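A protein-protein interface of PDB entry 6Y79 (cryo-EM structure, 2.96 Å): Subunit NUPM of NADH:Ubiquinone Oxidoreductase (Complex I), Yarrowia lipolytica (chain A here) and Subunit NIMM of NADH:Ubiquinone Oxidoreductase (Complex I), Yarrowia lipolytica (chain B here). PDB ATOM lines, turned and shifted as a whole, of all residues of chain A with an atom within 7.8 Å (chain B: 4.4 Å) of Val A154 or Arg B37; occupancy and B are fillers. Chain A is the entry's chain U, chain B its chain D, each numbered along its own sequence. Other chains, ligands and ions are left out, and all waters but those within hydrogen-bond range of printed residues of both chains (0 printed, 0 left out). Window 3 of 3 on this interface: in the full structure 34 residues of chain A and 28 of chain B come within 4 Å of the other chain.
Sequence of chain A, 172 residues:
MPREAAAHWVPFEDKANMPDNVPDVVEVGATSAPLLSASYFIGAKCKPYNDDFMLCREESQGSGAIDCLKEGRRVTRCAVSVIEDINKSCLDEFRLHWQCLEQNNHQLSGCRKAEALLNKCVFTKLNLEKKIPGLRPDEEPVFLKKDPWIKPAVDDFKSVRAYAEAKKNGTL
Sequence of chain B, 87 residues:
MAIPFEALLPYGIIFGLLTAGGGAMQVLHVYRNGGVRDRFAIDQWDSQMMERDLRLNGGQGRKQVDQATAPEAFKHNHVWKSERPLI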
ATOM      1  N   CYS A 100     -11.997 -31.630  -6.785  1.00  0.00           N
ATOM      2  CA  CYS A 100     -11.401 -30.791  -5.747  1.00  0.00           C
ATOM      3  C   CYS A 100      -9.941 -30.491  -6.066  1.00  0.00           C
ATOM      4  O   CYS A 100      -9.477 -29.365  -5.869  1.00  0.00           O
ATOM      5  CB  CYS A 100     -11.516 -31.467  -4.377  1.00  0.00           C
ATOM      6  SG  CYS A 100     -10.832 -30.554  -2.953  1.00  0.00           S
ATOM      7  N   GLU A 102      -8.270 -30.185  -8.854  1.00  0.00           N
ATOM      8  CA  GLU A 102      -7.858 -29.296  -9.939  1.00  0.00           C
ATOM      9  C   GLU A 102      -7.961 -27.831  -9.570  1.00  0.00           C
ATOM     10  O   GLU A 102      -7.314 -26.986 -10.196  1.00  0.00           O
ATOM     11  CB  GLU A 102      -8.653 -29.573 -11.183  1.00  0.00           C
ATOM     12  CG  GLU A 102     -10.112 -29.332 -11.247  1.00  0.00           C
ATOM     13  CD  GLU A 102     -10.634 -29.833 -12.611  1.00  0.00           C
ATOM     14  OE1 GLU A 102      -9.770 -30.349 -13.344  1.00  0.00           O
ATOM     15  OE2 GLU A 102     -11.805 -29.705 -12.892  1.00  0.00           O
ATOM     16  N   GLN A 103      -8.755 -27.504  -8.560  1.00  0.00           N
ATOM     17  CA  GLN A 103      -8.523 -26.264  -7.851  1.00  0.00           C
ATOM     18  C   GLN A 103      -7.437 -26.526  -6.819  1.00  0.00           C
ATOM     19  O   GLN A 103      -7.011 -27.664  -6.630  1.00  0.00           O
ATOM     20  CB  GLN A 103      -9.793 -25.742  -7.196  1.00  0.00           C
ATOM     21  CG  GLN A 103     -10.774 -25.093  -8.140  1.00  0.00           C
ATOM     22  CD  GLN A 103     -11.864 -26.029  -8.548  1.00  0.00           C
ATOM     23  OE1 GLN A 103     -12.020 -27.095  -7.965  1.00  0.00           O
ATOM     24  NE2 GLN A 103     -12.645 -25.636  -9.541  1.00  0.00           N
ATOM     25  N   ASN A 104      -6.980 -25.459  -6.156  1.00  0.00           N
ATOM     26  CA  ASN A 104      -6.010 -25.525  -5.053  1.00  0.00           C
ATOM     27  C   ASN A 104      -4.664 -26.113  -5.473  1.00  0.00           C
ATOM     28  O   ASN A 104      -4.057 -26.853  -4.707  1.00  0.00           O
ATOM     29  CB  ASN A 104      -6.561 -26.310  -3.854  1.00  0.00           C
ATOM     30  CG  ASN A 104      -7.713 -25.621  -3.180  1.00  0.00           C
ATOM     31  OD1 ASN A 104      -7.699 -24.408  -2.972  1.00  0.00           O
ATOM     32  ND2 ASN A 104      -8.724 -26.397  -2.822  1.00  0.00           N
ATOM     33  N   ASN A 105      -4.209 -25.802  -6.699  1.00  0.00           N
ATOM     34  CA  ASN A 105      -2.825 -26.044  -7.160  1.00  0.00           C
ATOM     35  C   ASN A 105      -2.410 -27.520  -7.088  1.00  0.00           C
ATOM     36  O   ASN A 105      -1.228 -27.835  -6.935  1.00  0.00           O
ATOM     37  CB  ASN A 105      -1.832 -25.171  -6.378  1.00  0.00           C
ATOM     38  CG  ASN A 105      -0.546 -24.911  -7.139  1.00  0.00           C
ATOM     39  OD1 ASN A 105      -0.430 -25.253  -8.313  1.00  0.00           O
ATOM     40  ND2 ASN A 105       0.439 -24.344  -6.462  1.00  0.00           N
ATOM     41  N   GLY A 110      -5.587 -29.550   0.618  1.00  0.00           N
ATOM     42  CA  GLY A 110      -6.855 -28.866   0.552  1.00  0.00           C
ATOM     43  C   GLY A 110      -8.049 -29.705   0.165  1.00  0.00           C
ATOM     44  O   GLY A 110      -9.079 -29.143  -0.212  1.00  0.00           O
ATOM     45  N   CYS A 111      -7.963 -31.022   0.233  1.00  0.00           N
ATOM     46  CA  CYS A 111      -9.037 -31.882  -0.240  1.00  0.00           C
ATOM     47  C   CYS A 111      -9.241 -33.049   0.713  1.00  0.00           C
ATOM     48  O   CYS A 111      -9.381 -34.198   0.302  1.00  0.00           O
ATOM     49  CB  CYS A 111      -8.751 -32.359  -1.654  1.00  0.00           C
ATOM     50  SG  CYS A 111      -8.848 -31.073  -2.908  1.00  0.00           S
ATOM     51  N   LYS A 151      -5.080 -25.653   6.703  1.00  0.00           N
ATOM     52  CA  LYS A 151      -6.399 -25.694   6.122  1.00  0.00           C
ATOM     53  C   LYS A 151      -6.383 -24.976   4.782  1.00  0.00           C
ATOM     54  O   LYS A 151      -5.571 -24.072   4.571  1.00  0.00           O
ATOM     55  CB  LYS A 151      -7.408 -25.021   7.053  1.00  0.00           C
ATOM     56  CG  LYS A 151      -7.493 -25.663   8.416  1.00  0.00           C
ATOM     57  CD  LYS A 151      -8.520 -24.974   9.280  1.00  0.00           C
ATOM     58  CE  LYS A 151      -8.691 -25.699  10.597  1.00  0.00           C
ATOM     59  NZ  LYS A 151      -9.686 -25.020  11.472  1.00  0.00           N
ATOM     60  N   PRO A 152      -7.229 -25.353   3.834  1.00  0.00           N
ATOM     61  CA  PRO A 152      -7.277 -24.631   2.563  1.00  0.00           C
ATOM     62  C   PRO A 152      -8.027 -23.314   2.696  1.00  0.00           C
ATOM     63  O   PRO A 152      -8.573 -22.973   3.745  1.00  0.00           O
ATOM     64  CB  PRO A 152      -8.010 -25.594   1.635  1.00  0.00           C
ATOM     65  CG  PRO A 152      -8.787 -26.443   2.520  1.00  0.00           C
ATOM     66  CD  PRO A 152      -8.010 -26.596   3.779  1.00  0.00           C
ATOM     67  N   ALA A 153      -8.025 -22.568   1.592  1.00  0.00           N
ATOM     68  CA  ALA A 153      -8.678 -21.267   1.566  1.00  0.00           C
ATOM     69  C   ALA A 153     -10.187 -21.411   1.656  1.00  0.00           C
ATOM     70  O   ALA A 153     -10.818 -20.875   2.573  1.00  0.00           O
ATOM     71  CB  ALA A 153      -8.289 -20.516   0.296  1.00  0.00           C
ATOM     72  N   VAL A 154     -10.787 -22.117   0.700  1.00  0.00           N
ATOM     73  CA  VAL A 154     -12.216 -22.409   0.687  1.00  0.00           C
ATOM     74  C   VAL A 154     -12.386 -23.902   0.446  1.00  0.00           C
ATOM     75  O   VAL A 154     -11.854 -24.433  -0.537  1.00  0.00           O
ATOM     76  CB  VAL A 154     -12.975 -21.615  -0.391  1.00  0.00           C
ATOM     77  CG1 VAL A 154     -14.458 -21.828  -0.230  1.00  0.00           C
ATOM     78  CG2 VAL A 154     -12.657 -20.131  -0.345  1.00  0.00           C
ATOM     79  N   ASP A 155     -13.111 -24.576   1.339  1.00  0.00           N
ATOM     80  CA  ASP A 155     -13.504 -25.956   1.092  1.00  0.00           C
ATOM     81  C   ASP A 155     -14.514 -26.023  -0.039  1.00  0.00           C
ATOM     82  O   ASP A 155     -15.414 -25.187  -0.130  1.00  0.00           O
ATOM     83  CB  ASP A 155     -14.096 -26.571   2.355  1.00  0.00           C
ATOM     84  CG  ASP A 155     -13.104 -26.613   3.492  1.00  0.00           C
ATOM     85  OD1 ASP A 155     -11.909 -26.722   3.183  1.00  0.00           O
ATOM     86  OD2 ASP A 155     -13.506 -26.552   4.671  1.00  0.00           O
ATOM     87  N   ASP A 156     -14.358 -27.022  -0.903  1.00  0.00           N
ATOM     88  CA  ASP A 156     -15.266 -27.204  -2.022  1.00  0.00           C
ATOM     89  C   ASP A 156     -16.648 -27.587  -1.507  1.00  0.00           C
ATOM     90  O   ASP A 156     -16.794 -28.281  -0.501  1.00  0.00           O
ATOM     91  CB  ASP A 156     -14.733 -28.274  -2.983  1.00  0.00           C
ATOM     92  CG  ASP A 156     -15.506 -28.344  -4.308  1.00  0.00           C
ATOM     93  OD1 ASP A 156     -16.505 -27.619  -4.506  1.00  0.00           O
ATOM     94  OD2 ASP A 156     -15.092 -29.135  -5.174  1.00  0.00           O
ATOM     95  N   PHE A 157     -17.666 -27.119  -2.227  1.00  0.00           N
ATOM     96  CA  PHE A 157     -19.030 -27.192  -1.724  1.00  0.00           C
ATOM     97  C   PHE A 157     -19.605 -28.593  -1.861  1.00  0.00           C
ATOM     98  O   PHE A 157     -20.288 -29.080  -0.950  1.00  0.00           O
ATOM     99  CB  PHE A 157     -19.888 -26.179  -2.465  1.00  0.00           C
ATOM    100  CG  PHE A 157     -19.438 -24.766  -2.284  1.00  0.00           C
ATOM    101  CD1 PHE A 157     -19.826 -24.053  -1.171  1.00  0.00           C
ATOM    102  CD2 PHE A 157     -18.630 -24.147  -3.224  1.00  0.00           C
ATOM    103  CE1 PHE A 157     -19.417 -22.755  -0.991  1.00  0.00           C
ATOM    104  CE2 PHE A 157     -18.218 -22.841  -3.046  1.00  0.00           C
ATOM    105  CZ  PHE A 157     -18.614 -22.147  -1.929  1.00  0.00           C
ATOM    106  N   SER A 159     -18.026 -31.430  -1.861  1.00  0.00           N
ATOM    107  CA  SER A 159     -17.416 -32.388  -0.955  1.00  0.00           C
ATOM    108  C   SER A 159     -17.814 -32.151   0.496  1.00  0.00           C
ATOM    109  O   SER A 159     -17.937 -33.117   1.249  1.00  0.00           O
ATOM    110  CB  SER A 159     -15.897 -32.368  -1.108  1.00  0.00           C
ATOM    111  OG  SER A 159     -15.356 -31.130  -0.701  1.00  0.00           O
ATOM    112  N   ASN B  33      -8.313 -19.603 -17.513  1.00  0.00           N
ATOM    113  CA  ASN B  33      -8.160 -21.030 -17.238  1.00  0.00           C
ATOM    114  C   ASN B  33      -9.360 -21.844 -17.701  1.00  0.00           C
ATOM    115  O   ASN B  33      -9.205 -23.008 -18.081  1.00  0.00           O
ATOM    116  CB  ASN B  33      -7.939 -21.270 -15.753  1.00  0.00           C
ATOM    117  CG  ASN B  33      -6.648 -20.699 -15.267  1.00  0.00           C
ATOM    118  OD1 ASN B  33      -6.625 -19.920 -14.323  1.00  0.00           O
ATOM    119  ND2 ASN B  33      -5.555 -21.074 -15.911  1.00  0.00           N
ATOM    120  N   VAL B  36     -11.427 -22.399 -13.381  1.00  0.00           N
ATOM    121  CA  VAL B  36     -10.682 -22.861 -12.220  1.00  0.00           C
ATOM    122  C   VAL B  36      -9.607 -21.834 -11.884  1.00  0.00           C
ATOM    123  O   VAL B  36      -9.381 -20.878 -12.622  1.00  0.00           O
ATOM    124  CB  VAL B  36     -10.055 -24.249 -12.440  1.00  0.00           C
ATOM    125  CG1 VAL B  36     -11.126 -25.307 -12.613  1.00  0.00           C
ATOM    126  CG2 VAL B  36      -9.163 -24.215 -13.639  1.00  0.00           C
ATOM    127  N   ARG B  37      -8.933 -22.053 -10.763  1.00  0.00           N
ATOM    128  CA  ARG B  37      -7.932 -21.124 -10.270  1.00  0.00           C
ATOM    129  C   ARG B  37      -6.585 -21.346 -10.953  1.00  0.00           C
ATOM    130  O   ARG B  37      -6.349 -22.355 -11.619  1.00  0.00           O
ATOM    131  CB  ARG B  37      -7.789 -21.263  -8.763  1.00  0.00           C
ATOM    132  CG  ARG B  37      -9.040 -20.903  -8.015  1.00  0.00           C
ATOM    133  CD  ARG B  37      -8.872 -21.155  -6.541  1.00  0.00           C
ATOM    134  NE  ARG B  37     -10.081 -20.829  -5.804  1.00  0.00           N
ATOM    135  CZ  ARG B  37     -10.245 -21.066  -4.510  1.00  0.00           C
ATOM    136  NH1 ARG B  37     -11.378 -20.735  -3.912  1.00  0.00           N
ATOM    137  NH2 ARG B  37      -9.275 -21.634  -3.810  1.00  0.00           N
ATOM    138  N   ASP B  38      -5.694 -20.374 -10.780  1.00  0.00           N
ATOM    139  CA  ASP B  38      -4.359 -20.475 -11.341  1.00  0.00           C
ATOM    140  C   ASP B  38      -3.495 -21.411 -10.509  1.00  0.00           C
ATOM    141  O   ASP B  38      -3.791 -21.718  -9.354  1.00  0.00           O
ATOM    142  CB  ASP B  38      -3.686 -19.106 -11.403  1.00  0.00           C
ATOM    143  CG  ASP B  38      -4.575 -18.043 -11.982  1.00  0.00           C
ATOM    144  OD1 ASP B  38      -4.766 -18.029 -13.215  1.00  0.00           O
ATOM    145  OD2 ASP B  38      -5.084 -17.218 -11.198  1.00  0.00           O
ATOM    146  N   ARG B  39      -2.402 -21.847 -11.112  1.00  0.00           N
ATOM    147  CA  ARG B  39      -1.381 -22.620 -10.426  1.00  0.00           C
ATOM    148  C   ARG B  39      -0.249 -21.669 -10.068  1.00  0.00           C
ATOM    149  O   ARG B  39       0.398 -21.107 -10.956  1.00  0.00           O
ATOM    150  CB  ARG B  39      -0.885 -23.750 -11.310  1.00  0.00           C
ATOM    151  CG  ARG B  39      -1.962 -24.654 -11.833  1.00  0.00           C
ATOM    152  CD  ARG B  39      -1.294 -25.724 -12.639  1.00  0.00           C
ATOM    153  NE  ARG B  39      -0.134 -26.192 -11.895  1.00  0.00           N
ATOM    154  CZ  ARG B  39      -0.056 -27.373 -11.307  1.00  0.00           C
ATOM    155  NH1 ARG B  39      -1.050 -28.221 -11.423  1.00  0.00           N
ATOM    156  NH2 ARG B  39       1.026 -27.710 -10.626  1.00  0.00           N
ATOM    157  N   ARG B  62      -6.540 -27.189 -19.466  1.00  0.00           N
ATOM    158  CA  ARG B  62      -6.620 -28.081 -18.313  1.00  0.00           C
ATOM    159  C   ARG B  62      -8.020 -28.674 -18.202  1.00  0.00           C
ATOM    160  O   ARG B  62      -8.688 -28.583 -17.171  1.00  0.00           O
ATOM    161  CB  ARG B  62      -6.175 -27.368 -17.037  1.00  0.00           C
ATOM    162  CG  ARG B  62      -6.741 -25.983 -16.806  1.00  0.00           C
ATOM    163  CD  ARG B  62      -6.151 -25.394 -15.535  1.00  0.00           C
ATOM    164  NE  ARG B  62      -6.365 -26.276 -14.393  1.00  0.00           N
ATOM    165  CZ  ARG B  62      -5.934 -26.024 -13.163  1.00  0.00           C
ATOM    166  NH1 ARG B  62      -6.164 -26.889 -12.193  1.00  0.00           N
ATOM    167  NH2 ARG B  62      -5.290 -24.900 -12.905  1.00  0.00           N
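The guanidinium group (NH2) of Arg B37 sits at hydrogen-bond distance from the side-chain amide oxygen (OD1) of Asn A104, at 3.3 Å.
The backbone carbonyl oxygen (O) of Glu A102 lies close to the guanidinium group (NH1) of Arg B62, 2.3 Å away.
The backbone carbonyl oxygen of Val B36 sits close to the side-chain amide oxygen of Asn B33.
O of Arg B37 lies within hydrogen-bond range of NH2 of Arg B62 (3.0 Å).
The side-chain sulfur of Cys A100 is disulfide-bonded to the side-chain sulfur of Cys A111, at 2.1 Å.
Among the printed residues, pairs that only touch across the chains: Asn A105 with Arg B39 (3.4 Å), Gln A103 with Val B36 (3.4 Å) and Val A154 with Arg B37 (3.8 Å).
Printed residues of chain B within 4 Å of Gln A103: Val B36 (3.4 Å).
Printed residues of chain B within 4 Å of Asn A104: Arg B37.
Of the printed residues of chain B, Asn A105 touches Arg B39 (3.4 Å).
Of chain B, only Arg B37 comes within 4 Å of Val A154.
Printed residues of chain A within 4 Å of Val B36: Gln A103 (3.4 Å).
Printed residues of chain A within 4 Å of Arg B37: Asn A104 (3.3 Å) and Val A154 (3.8 Å).
Asp B38 touches none of the printed residues of chain A.
Printed residues of chain A within 4 Å of Arg B62: Glu A102.
The nearest residue of chain A that does not touch Arg B37 is Ala A153 (4.4 Å).
Printed residues of chain A that touch a printed residue of chain B: Glu A102, Gln A103, Asn A104, Asn A105 and Val A154.
Hydrophobic or aromatic side chains of chain B within 4 Å of the printed part of chain A: Val B36.
Along chain B the printed residues that touch a printed residue of chain A span positions 36 to 62.
Among the printed residues, 5 pairs touch across the chains.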
